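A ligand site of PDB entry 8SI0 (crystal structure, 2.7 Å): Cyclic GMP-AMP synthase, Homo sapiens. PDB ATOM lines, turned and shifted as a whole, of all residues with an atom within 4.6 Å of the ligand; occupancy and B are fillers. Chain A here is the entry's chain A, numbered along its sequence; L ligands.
N7 of the ligand lies within hydrogen-bond range of NH2 of Arg 223 (2.8 Å). The side-chain amino group (NZ) of Lys 209 lies within salt-bridge range of an oxygen (O9) of the ligand (3.7 Å). O5 of the ligand sits at hydrogen-bond distance from NH1 of Arg 149, at 2.9 Å. OD2 of Asp 166 is in hydrogen-bond range of N9 of the ligand (3.0 Å). The side-chain carboxylate of Asp 74 is in hydrogen-bond range of a nitrogen (N9) of the ligand (3.0 Å). OG of Ser 281 lies close to O3 of the ligand. A nitrogen (N1) of the ligand lies within hydrogen-bond range of the side-chain hydroxyl of Ser 227 (3.2 Å).
The backbone carbonyl oxygen (O) of Arg 223 lies within hydrogen-bond range of the backbone NH (N) of Val 207, 2.9 Å away. The backbone NH (N) of Ala 154 sits at hydrogen-bond distance from the side-chain hydroxyl (OG) of Ser 152 (3.2 Å). N of Ser 281 is in hydrogen-bond range of ND1 of His 284, at 3.0 Å. The side-chain hydroxyl (OG) of Ser 227 is in hydrogen-bond range of the side-chain hydroxyl (OG) of Ser 225 (3.2 Å).
Merely in contact with the ligand: Ser 152 (3.1 Å), Tyr 283 (3.3 Å), Pro 153 (3.7 Å), Ser 225 (3.7 Å), Leu 342 (3.8 Å), Leu 337 (3.9 Å) and His 284 (3.9999 Å). Within 4 Å of the ligand: Asp 74, Arg 149, Ser 152, Pro 153, Asp 166, Lys 209, Arg 223, Ser 225, Ser 227, Ser 281, Tyr 283, His 284, Leu 337 and Leu 342.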
ATOM      1  N   ASP A  74     -30.765  -8.687   4.397  1.00  0.00           N
ATOM      2  CA  ASP A  74     -30.128  -9.782   3.666  1.00  0.00           C
ATOM      3  C   ASP A  74     -30.576  -9.765   2.197  1.00  0.00           C
ATOM      4  O   ASP A  74     -31.764  -9.956   1.916  1.00  0.00           O
ATOM      5  CB  ASP A  74     -30.455 -11.114   4.335  1.00  0.00           C
ATOM      6  CG  ASP A  74     -30.179 -12.268   3.430  1.00  0.00           C
ATOM      7  OD1 ASP A  74     -28.978 -12.661   3.296  1.00  0.00           O
ATOM      8  OD2 ASP A  74     -31.167 -12.744   2.814  1.00  0.00           O
ATOM      9  N   TYR A  95     -22.576 -29.217   2.825  1.00  0.00           N
ATOM     10  CA  TYR A  95     -21.406 -28.567   2.218  1.00  0.00           C
ATOM     11  C   TYR A  95     -20.821 -29.430   1.108  1.00  0.00           C
ATOM     12  O   TYR A  95     -20.703 -30.650   1.243  1.00  0.00           O
ATOM     13  CB  TYR A  95     -20.334 -28.271   3.260  1.00  0.00           C
ATOM     14  CG  TYR A  95     -20.759 -27.355   4.389  1.00  0.00           C
ATOM     15  CD1 TYR A  95     -21.466 -27.835   5.482  1.00  0.00           C
ATOM     16  CD2 TYR A  95     -20.400 -26.004   4.392  1.00  0.00           C
ATOM     17  CE1 TYR A  95     -21.843 -27.000   6.524  1.00  0.00           C
ATOM     18  CE2 TYR A  95     -20.775 -25.159   5.438  1.00  0.00           C
ATOM     19  CZ  TYR A  95     -21.488 -25.669   6.502  1.00  0.00           C
ATOM     20  OH  TYR A  95     -21.861 -24.850   7.529  1.00  0.00           O
ATOM     21  N   ARG A 149     -18.073 -11.832  10.335  1.00  0.00           N
ATOM     22  CA  ARG A 149     -17.774 -13.063  11.056  1.00  0.00           C
ATOM     23  C   ARG A 149     -17.056 -14.047  10.143  1.00  0.00           C
ATOM     24  O   ARG A 149     -17.133 -13.965   8.904  1.00  0.00           O
ATOM     25  CB  ARG A 149     -19.053 -13.710  11.623  1.00  0.00           C
ATOM     26  CG  ARG A 149     -19.810 -12.815  12.604  1.00  0.00           C
ATOM     27  CD  ARG A 149     -20.785 -13.616  13.451  1.00  0.00           C
ATOM     28  NE  ARG A 149     -20.093 -14.536  14.340  1.00  0.00           N
ATOM     29  CZ  ARG A 149     -20.179 -15.859  14.263  1.00  0.00           C
ATOM     30  NH1 ARG A 149     -20.925 -16.442  13.343  1.00  0.00           N
ATOM     31  NH2 ARG A 149     -19.499 -16.610  15.124  1.00  0.00           N
ATOM     32  N   GLY A 150     -16.335 -14.977  10.765  1.00  0.00           N
ATOM     33  CA  GLY A 150     -15.797 -16.117  10.050  1.00  0.00           C
ATOM     34  C   GLY A 150     -16.865 -17.144   9.740  1.00  0.00           C
ATOM     35  O   GLY A 150     -17.910 -17.232  10.402  1.00  0.00           O
ATOM     36  N   GLY A 151     -16.596 -17.944   8.711  1.00  0.00           N
ATOM     37  CA  GLY A 151     -17.596 -18.842   8.180  1.00  0.00           C
ATOM     38  C   GLY A 151     -18.409 -18.185   7.082  1.00  0.00           C
ATOM     39  O   GLY A 151     -18.315 -18.593   5.911  1.00  0.00           O
ATOM     40  N   SER A 152     -19.175 -17.128   7.446  1.00  0.00           N
ATOM     41  CA  SER A 152     -20.231 -16.432   6.706  1.00  0.00           C
ATOM     42  C   SER A 152     -19.915 -16.151   5.239  1.00  0.00           C
ATOM     43  O   SER A 152     -18.803 -15.724   4.912  1.00  0.00           O
ATOM     44  CB  SER A 152     -20.569 -15.095   7.373  1.00  0.00           C
ATOM     45  OG  SER A 152     -21.621 -14.434   6.687  1.00  0.00           O
ATOM     46  N   PRO A 153     -20.873 -16.353   4.341  1.00  0.00           N
ATOM     47  CA  PRO A 153     -20.689 -16.017   2.926  1.00  0.00           C
ATOM     48  C   PRO A 153     -21.125 -14.616   2.577  1.00  0.00           C
ATOM     49  O   PRO A 153     -21.019 -14.199   1.411  1.00  0.00           O
ATOM     50  CB  PRO A 153     -21.576 -17.060   2.227  1.00  0.00           C
ATOM     51  CG  PRO A 153     -22.715 -17.243   3.193  1.00  0.00           C
ATOM     52  CD  PRO A 153     -22.210 -16.916   4.589  1.00  0.00           C
ATOM     53  N   ALA A 154     -21.620 -13.877   3.558  1.00  0.00           N
ATOM     54  CA  ALA A 154     -22.162 -12.550   3.344  1.00  0.00           C
ATOM     55  C   ALA A 154     -21.060 -11.499   3.388  1.00  0.00           C
ATOM     56  O   ALA A 154     -20.291 -11.431   4.362  1.00  0.00           O
ATOM     57  CB  ALA A 154     -23.237 -12.245   4.385  1.00  0.00           C
ATOM     58  N   ASP A 166     -26.592  -7.657   4.483  1.00  0.00           N
ATOM     59  CA  ASP A 166     -25.815  -8.843   4.155  1.00  0.00           C
ATOM     60  C   ASP A 166     -26.019  -9.139   2.671  1.00  0.00           C
ATOM     61  O   ASP A 166     -27.102  -9.599   2.282  1.00  0.00           O
ATOM     62  CB  ASP A 166     -26.272 -10.037   4.989  1.00  0.00           C
ATOM     63  CG  ASP A 166     -25.471 -10.220   6.271  1.00  0.00           C
ATOM     64  OD1 ASP A 166     -25.080  -9.208   6.883  1.00  0.00           O
ATOM     65  OD2 ASP A 166     -25.268 -11.383   6.672  1.00  0.00           O
ATOM     66  N   THR A 168     -25.018 -11.644  -0.179  1.00  0.00           N
ATOM     67  CA  THR A 168     -24.516 -12.997  -0.293  1.00  0.00           C
ATOM     68  C   THR A 168     -24.570 -13.444  -1.747  1.00  0.00           C
ATOM     69  O   THR A 168     -25.638 -13.470  -2.347  1.00  0.00           O
ATOM     70  CB  THR A 168     -25.332 -13.971   0.559  1.00  0.00           C
ATOM     71  OG1 THR A 168     -25.533 -13.414   1.862  1.00  0.00           O
ATOM     72  CG2 THR A 168     -24.603 -15.263   0.669  1.00  0.00           C
ATOM     73  N   VAL A 207     -23.974 -21.120  -1.604  1.00  0.00           N
ATOM     74  CA  VAL A 207     -23.361 -19.906  -1.061  1.00  0.00           C
ATOM     75  C   VAL A 207     -21.964 -20.269  -0.584  1.00  0.00           C
ATOM     76  O   VAL A 207     -21.783 -21.347   0.008  1.00  0.00           O
ATOM     77  CB  VAL A 207     -24.208 -19.307   0.075  1.00  0.00           C
ATOM     78  CG1 VAL A 207     -25.339 -18.496  -0.494  1.00  0.00           C
ATOM     79  CG2 VAL A 207     -24.767 -20.401   0.973  1.00  0.00           C
ATOM     80  N   LYS A 209     -20.133 -20.409   1.852  1.00  0.00           N
ATOM     81  CA  LYS A 209     -19.899 -20.638   3.262  1.00  0.00           C
ATOM     82  C   LYS A 209     -19.186 -21.975   3.329  1.00  0.00           C
ATOM     83  O   LYS A 209     -19.670 -22.956   2.759  1.00  0.00           O
ATOM     84  CB  LYS A 209     -21.219 -20.640   4.040  1.00  0.00           C
ATOM     85  CG  LYS A 209     -21.060 -20.435   5.498  1.00  0.00           C
ATOM     86  CD  LYS A 209     -20.885 -21.760   6.152  1.00  0.00           C
ATOM     87  CE  LYS A 209     -20.966 -21.639   7.645  1.00  0.00           C
ATOM     88  NZ  LYS A 209     -19.655 -21.552   8.339  1.00  0.00           N
ATOM     89  N   ARG A 223     -22.050 -24.213   0.419  1.00  0.00           N
ATOM     90  CA  ARG A 223     -23.132 -24.952   1.067  1.00  0.00           C
ATOM     91  C   ARG A 223     -24.479 -24.562   0.487  1.00  0.00           C
ATOM     92  O   ARG A 223     -24.659 -23.482  -0.088  1.00  0.00           O
ATOM     93  CB  ARG A 223     -23.142 -24.747   2.568  1.00  0.00           C
ATOM     94  CG  ARG A 223     -23.969 -23.593   3.012  1.00  0.00           C
ATOM     95  CD  ARG A 223     -24.848 -24.042   4.153  1.00  0.00           C
ATOM     96  NE  ARG A 223     -25.190 -22.933   5.037  1.00  0.00           N
ATOM     97  CZ  ARG A 223     -26.012 -21.948   4.706  1.00  0.00           C
ATOM     98  NH1 ARG A 223     -26.593 -21.900   3.517  1.00  0.00           N
ATOM     99  NH2 ARG A 223     -26.246 -20.981   5.592  1.00  0.00           N
ATOM    100  N   LEU A 224     -25.432 -25.483   0.618  1.00  0.00           N
ATOM    101  CA  LEU A 224     -26.734 -25.341  -0.022  1.00  0.00           C
ATOM    102  C   LEU A 224     -27.513 -24.213   0.613  1.00  0.00           C
ATOM    103  O   LEU A 224     -27.337 -23.910   1.791  1.00  0.00           O
ATOM    104  CB  LEU A 224     -27.538 -26.631   0.084  1.00  0.00           C
ATOM    105  CG  LEU A 224     -27.000 -27.777  -0.765  1.00  0.00           C
ATOM    106  CD1 LEU A 224     -27.547 -29.091  -0.278  1.00  0.00           C
ATOM    107  CD2 LEU A 224     -27.414 -27.509  -2.193  1.00  0.00           C
ATOM    108  N   SER A 225     -28.368 -23.586  -0.199  1.00  0.00           N
ATOM    109  CA  SER A 225     -29.357 -22.607   0.281  1.00  0.00           C
ATOM    110  C   SER A 225     -30.646 -22.755  -0.509  1.00  0.00           C
ATOM    111  O   SER A 225     -30.636 -23.105  -1.679  1.00  0.00           O
ATOM    112  CB  SER A 225     -28.866 -21.160   0.167  1.00  0.00           C
ATOM    113  OG  SER A 225     -29.867 -20.254   0.615  1.00  0.00           O
ATOM    114  N   SER A 227     -33.310 -20.188   0.238  1.00  0.00           N
ATOM    115  CA  SER A 227     -34.019 -19.040   0.775  1.00  0.00           C
ATOM    116  C   SER A 227     -35.180 -18.658  -0.112  1.00  0.00           C
ATOM    117  O   SER A 227     -36.169 -18.052   0.359  1.00  0.00           O
ATOM    118  CB  SER A 227     -33.051 -17.865   0.916  1.00  0.00           C
ATOM    119  OG  SER A 227     -32.020 -18.171   1.834  1.00  0.00           O
ATOM    120  N   LYS A 279     -25.120 -16.981  19.419  1.00  0.00           N
ATOM    121  CA  LYS A 279     -25.132 -18.018  18.388  1.00  0.00           C
ATOM    122  C   LYS A 279     -26.536 -18.282  17.831  1.00  0.00           C
ATOM    123  O   LYS A 279     -26.673 -18.760  16.709  1.00  0.00           O
ATOM    124  CB  LYS A 279     -24.533 -19.304  18.938  1.00  0.00           C
ATOM    125  CG  LYS A 279     -23.047 -19.243  19.293  1.00  0.00           C
ATOM    126  CD  LYS A 279     -22.190 -19.417  18.042  1.00  0.00           C
ATOM    127  CE  LYS A 279     -20.716 -19.656  18.382  1.00  0.00           C
ATOM    128  NZ  LYS A 279     -19.945 -20.024  17.152  1.00  0.00           N
ATOM    129  N   SER A 281     -30.190 -17.417  16.200  1.00  0.00           N
ATOM    130  CA  SER A 281     -30.596 -16.465  15.177  1.00  0.00           C
ATOM    131  C   SER A 281     -32.004 -16.772  14.694  1.00  0.00           C
ATOM    132  O   SER A 281     -32.564 -17.834  14.967  1.00  0.00           O
ATOM    133  CB  SER A 281     -29.633 -16.482  14.005  1.00  0.00           C
ATOM    134  OG  SER A 281     -29.779 -17.697  13.303  1.00  0.00           O
ATOM    135  N   TYR A 283     -32.988 -17.617  11.849  1.00  0.00           N
ATOM    136  CA  TYR A 283     -33.090 -18.839  11.045  1.00  0.00           C
ATOM    137  C   TYR A 283     -33.544 -20.021  11.900  1.00  0.00           C
ATOM    138  O   TYR A 283     -34.399 -20.804  11.477  1.00  0.00           O
ATOM    139  CB  TYR A 283     -31.752 -19.171  10.392  1.00  0.00           C
ATOM    140  CG  TYR A 283     -31.918 -20.107   9.240  1.00  0.00           C
ATOM    141  CD1 TYR A 283     -32.423 -19.653   8.029  1.00  0.00           C
ATOM    142  CD2 TYR A 283     -31.612 -21.453   9.363  1.00  0.00           C
ATOM    143  CE1 TYR A 283     -32.596 -20.515   6.963  1.00  0.00           C
ATOM    144  CE2 TYR A 283     -31.778 -22.319   8.303  1.00  0.00           C
ATOM    145  CZ  TYR A 283     -32.273 -21.850   7.106  1.00  0.00           C
ATOM    146  OH  TYR A 283     -32.446 -22.718   6.053  1.00  0.00           O
ATOM    147  N   HIS A 284     -32.964 -20.170  13.091  1.00  0.00           N
ATOM    148  CA  HIS A 284     -33.428 -21.208  14.001  1.00  0.00           C
ATOM    149  C   HIS A 284     -34.925 -21.087  14.241  1.00  0.00           C
ATOM    150  O   HIS A 284     -35.683 -22.051  14.066  1.00  0.00           O
ATOM    151  CB  HIS A 284     -32.635 -21.126  15.313  1.00  0.00           C
ATOM    152  CG  HIS A 284     -31.162 -21.275  15.144  1.00  0.00           C
ATOM    153  ND1 HIS A 284     -30.261 -20.340  15.581  1.00  0.00           N
ATOM    154  CD2 HIS A 284     -30.422 -22.255  14.565  1.00  0.00           C
ATOM    155  CE1 HIS A 284     -29.036 -20.720  15.282  1.00  0.00           C
ATOM    156  NE2 HIS A 284     -29.107 -21.888  14.672  1.00  0.00           N
ATOM    157  N   ASN A 329     -32.322 -28.969   9.706  1.00  0.00           N
ATOM    158  CA  ASN A 329     -32.559 -28.176   8.525  1.00  0.00           C
ATOM    159  C   ASN A 329     -33.769 -28.705   7.765  1.00  0.00           C
ATOM    160  O   ASN A 329     -33.838 -29.884   7.404  1.00  0.00           O
ATOM    161  CB  ASN A 329     -31.318 -28.199   7.658  1.00  0.00           C
ATOM    162  CG  ASN A 329     -31.435 -27.321   6.464  1.00  0.00           C
ATOM    163  OD1 ASN A 329     -32.177 -27.637   5.514  1.00  0.00           O
ATOM    164  ND2 ASN A 329     -30.752 -26.204   6.496  1.00  0.00           N
ATOM    165  N   PHE A 335     -28.727 -32.565   8.641  1.00  0.00           N
ATOM    166  CA  PHE A 335     -27.885 -31.446   9.033  1.00  0.00           C
ATOM    167  C   PHE A 335     -28.501 -30.821  10.271  1.00  0.00           C
ATOM    168  O   PHE A 335     -29.576 -30.204  10.197  1.00  0.00           O
ATOM    169  CB  PHE A 335     -27.725 -30.419   7.918  1.00  0.00           C
ATOM    170  CG  PHE A 335     -26.757 -29.353   8.282  1.00  0.00           C
ATOM    171  CD1 PHE A 335     -25.409 -29.643   8.358  1.00  0.00           C
ATOM    172  CD2 PHE A 335     -27.187 -28.119   8.663  1.00  0.00           C
ATOM    173  CE1 PHE A 335     -24.507 -28.685   8.742  1.00  0.00           C
ATOM    174  CE2 PHE A 335     -26.279 -27.169   9.037  1.00  0.00           C
ATOM    175  CZ  PHE A 335     -24.932 -27.456   9.083  1.00  0.00           C
ATOM    176  N   LEU A 337     -28.679 -28.177  12.930  1.00  0.00           N
ATOM    177  CA  LEU A 337     -28.345 -26.807  13.280  1.00  0.00           C
ATOM    178  C   LEU A 337     -28.011 -26.637  14.751  1.00  0.00           C
ATOM    179  O   LEU A 337     -27.494 -25.581  15.138  1.00  0.00           O
ATOM    180  CB  LEU A 337     -29.508 -25.884  12.898  1.00  0.00           C
ATOM    181  CG  LEU A 337     -29.908 -25.882  11.416  1.00  0.00           C
ATOM    182  CD1 LEU A 337     -31.171 -25.048  11.202  1.00  0.00           C
ATOM    183  CD2 LEU A 337     -28.783 -25.355  10.554  1.00  0.00           C
ATOM    184  N   LEU A 342     -21.842 -26.644  16.330  1.00  0.00           N
ATOM    185  CA  LEU A 342     -22.237 -25.272  16.031  1.00  0.00           C
ATOM    186  C   LEU A 342     -22.493 -24.457  17.298  1.00  0.00           C
ATOM    187  O   LEU A 342     -21.931 -23.372  17.475  1.00  0.00           O
ATOM    188  CB  LEU A 342     -23.502 -25.291  15.167  1.00  0.00           C
ATOM    189  CG  LEU A 342     -23.298 -25.948  13.813  1.00  0.00           C
ATOM    190  CD1 LEU A 342     -24.612 -26.028  13.029  1.00  0.00           C
ATOM    191  CD2 LEU A 342     -22.248 -25.191  13.034  1.00  0.00           C
HETATM  192  C1  LIG L   1     -29.263 -22.191   5.410  1.00  0.00           C
HETATM  193  N1  LIG L   1     -29.856 -18.992   4.104  1.00  0.00           N
HETATM  194  C2  LIG L   1     -29.461 -19.880   5.162  1.00  0.00           C
HETATM  195  N2  LIG L   1     -29.565 -21.112   4.661  1.00  0.00           N
HETATM  196  N3  LIG L   1     -28.854 -21.993   6.686  1.00  0.00           N
HETATM  197  C3  LIG L   1     -28.748 -20.757   7.204  1.00  0.00           C
HETATM  198  C4  LIG L   1     -29.037 -19.687   6.467  1.00  0.00           C
HETATM  199  N4  LIG L   1     -28.829 -18.593   7.219  1.00  0.00           N
HETATM  200  C5  LIG L   1     -28.416 -18.999   8.432  1.00  0.00           C
HETATM  201  N5  LIG L   1     -28.354 -20.352   8.415  1.00  0.00           N
HETATM  202  C6  LIG L   1     -27.933 -21.141   9.540  1.00  0.00           C
HETATM  203  C7  LIG L   1     -26.433 -21.385   9.477  1.00  0.00           C
HETATM  204  O1  LIG L   1     -26.143 -22.783   9.423  1.00  0.00           O
HETATM  205  C8  LIG L   1     -25.845 -20.741  10.674  1.00  0.00           C
HETATM  206  C9  LIG L   1     -26.975 -20.521  11.576  1.00  0.00           C
HETATM  207  C10 LIG L   1     -26.795 -19.119  12.215  1.00  0.00           C
HETATM  208  O2  LIG L   1     -26.709 -18.160  11.107  1.00  0.00           O
HETATM  209  P1  LIG L   1     -26.627 -16.471  11.435  1.00  0.00           P
HETATM  210  O3  LIG L   1     -27.978 -15.782  11.356  1.00  0.00           O
HETATM  211  O4  LIG L   1     -25.396 -15.709  10.524  1.00  0.00           O
HETATM  212  C11 LIG L   1     -24.350 -16.728  10.213  1.00  0.00           C
HETATM  213  C12 LIG L   1     -23.264 -16.698  11.201  1.00  0.00           C
HETATM  214  O5  LIG L   1     -22.940 -15.340  11.507  1.00  0.00           O
HETATM  215  C13 LIG L   1     -22.094 -17.312  10.475  1.00  0.00           C
HETATM  216  C14 LIG L   1     -21.944 -18.771  10.715  1.00  0.00           C
HETATM  217  O6  LIG L   1     -23.195 -19.406  11.195  1.00  0.00           O
HETATM  218  P2  LIG L   1     -23.188 -21.056  10.793  1.00  0.00           P
HETATM  219  O7  LIG L   1     -24.782 -21.552  11.318  1.00  0.00           O
HETATM  220  O8  LIG L   1     -23.248 -21.204   9.292  1.00  0.00           O
HETATM  221  O9  LIG L   1     -21.972 -21.838  11.238  1.00  0.00           O
HETATM  222  O10 LIG L   1     -22.358 -17.045   9.042  1.00  0.00           O
HETATM  223  C15 LIG L   1     -23.684 -16.437   9.013  1.00  0.00           C
HETATM  224  N6  LIG L   1     -24.412 -17.014   7.819  1.00  0.00           N
HETATM  225  C16 LIG L   1     -24.247 -18.310   7.482  1.00  0.00           C
HETATM  226  N7  LIG L   1     -24.992 -18.554   6.370  1.00  0.00           N
HETATM  227  C17 LIG L   1     -25.245 -16.453   6.925  1.00  0.00           C
HETATM  228  C18 LIG L   1     -25.606 -17.424   6.030  1.00  0.00           C
HETATM  229  C19 LIG L   1     -26.572 -17.093   4.878  1.00  0.00           C
HETATM  230  N8  LIG L   1     -27.086 -15.755   4.755  1.00  0.00           N
HETATM  231  C20 LIG L   1     -26.694 -14.738   5.709  1.00  0.00           C
HETATM  232  N9  LIG L   1     -27.206 -13.382   5.593  1.00  0.00           N
HETATM  233  N10 LIG L   1     -25.773 -15.058   6.802  1.00  0.00           N
HETATM  234  O11 LIG L   1     -26.874 -17.950   4.104  1.00  0.00           O
HETATM  235  O12 LIG L   1     -26.195 -16.351  12.879  1.00  0.00           O
HETATM  236  O13 LIG L   1     -28.210 -20.512  10.810  1.00  0.00           O
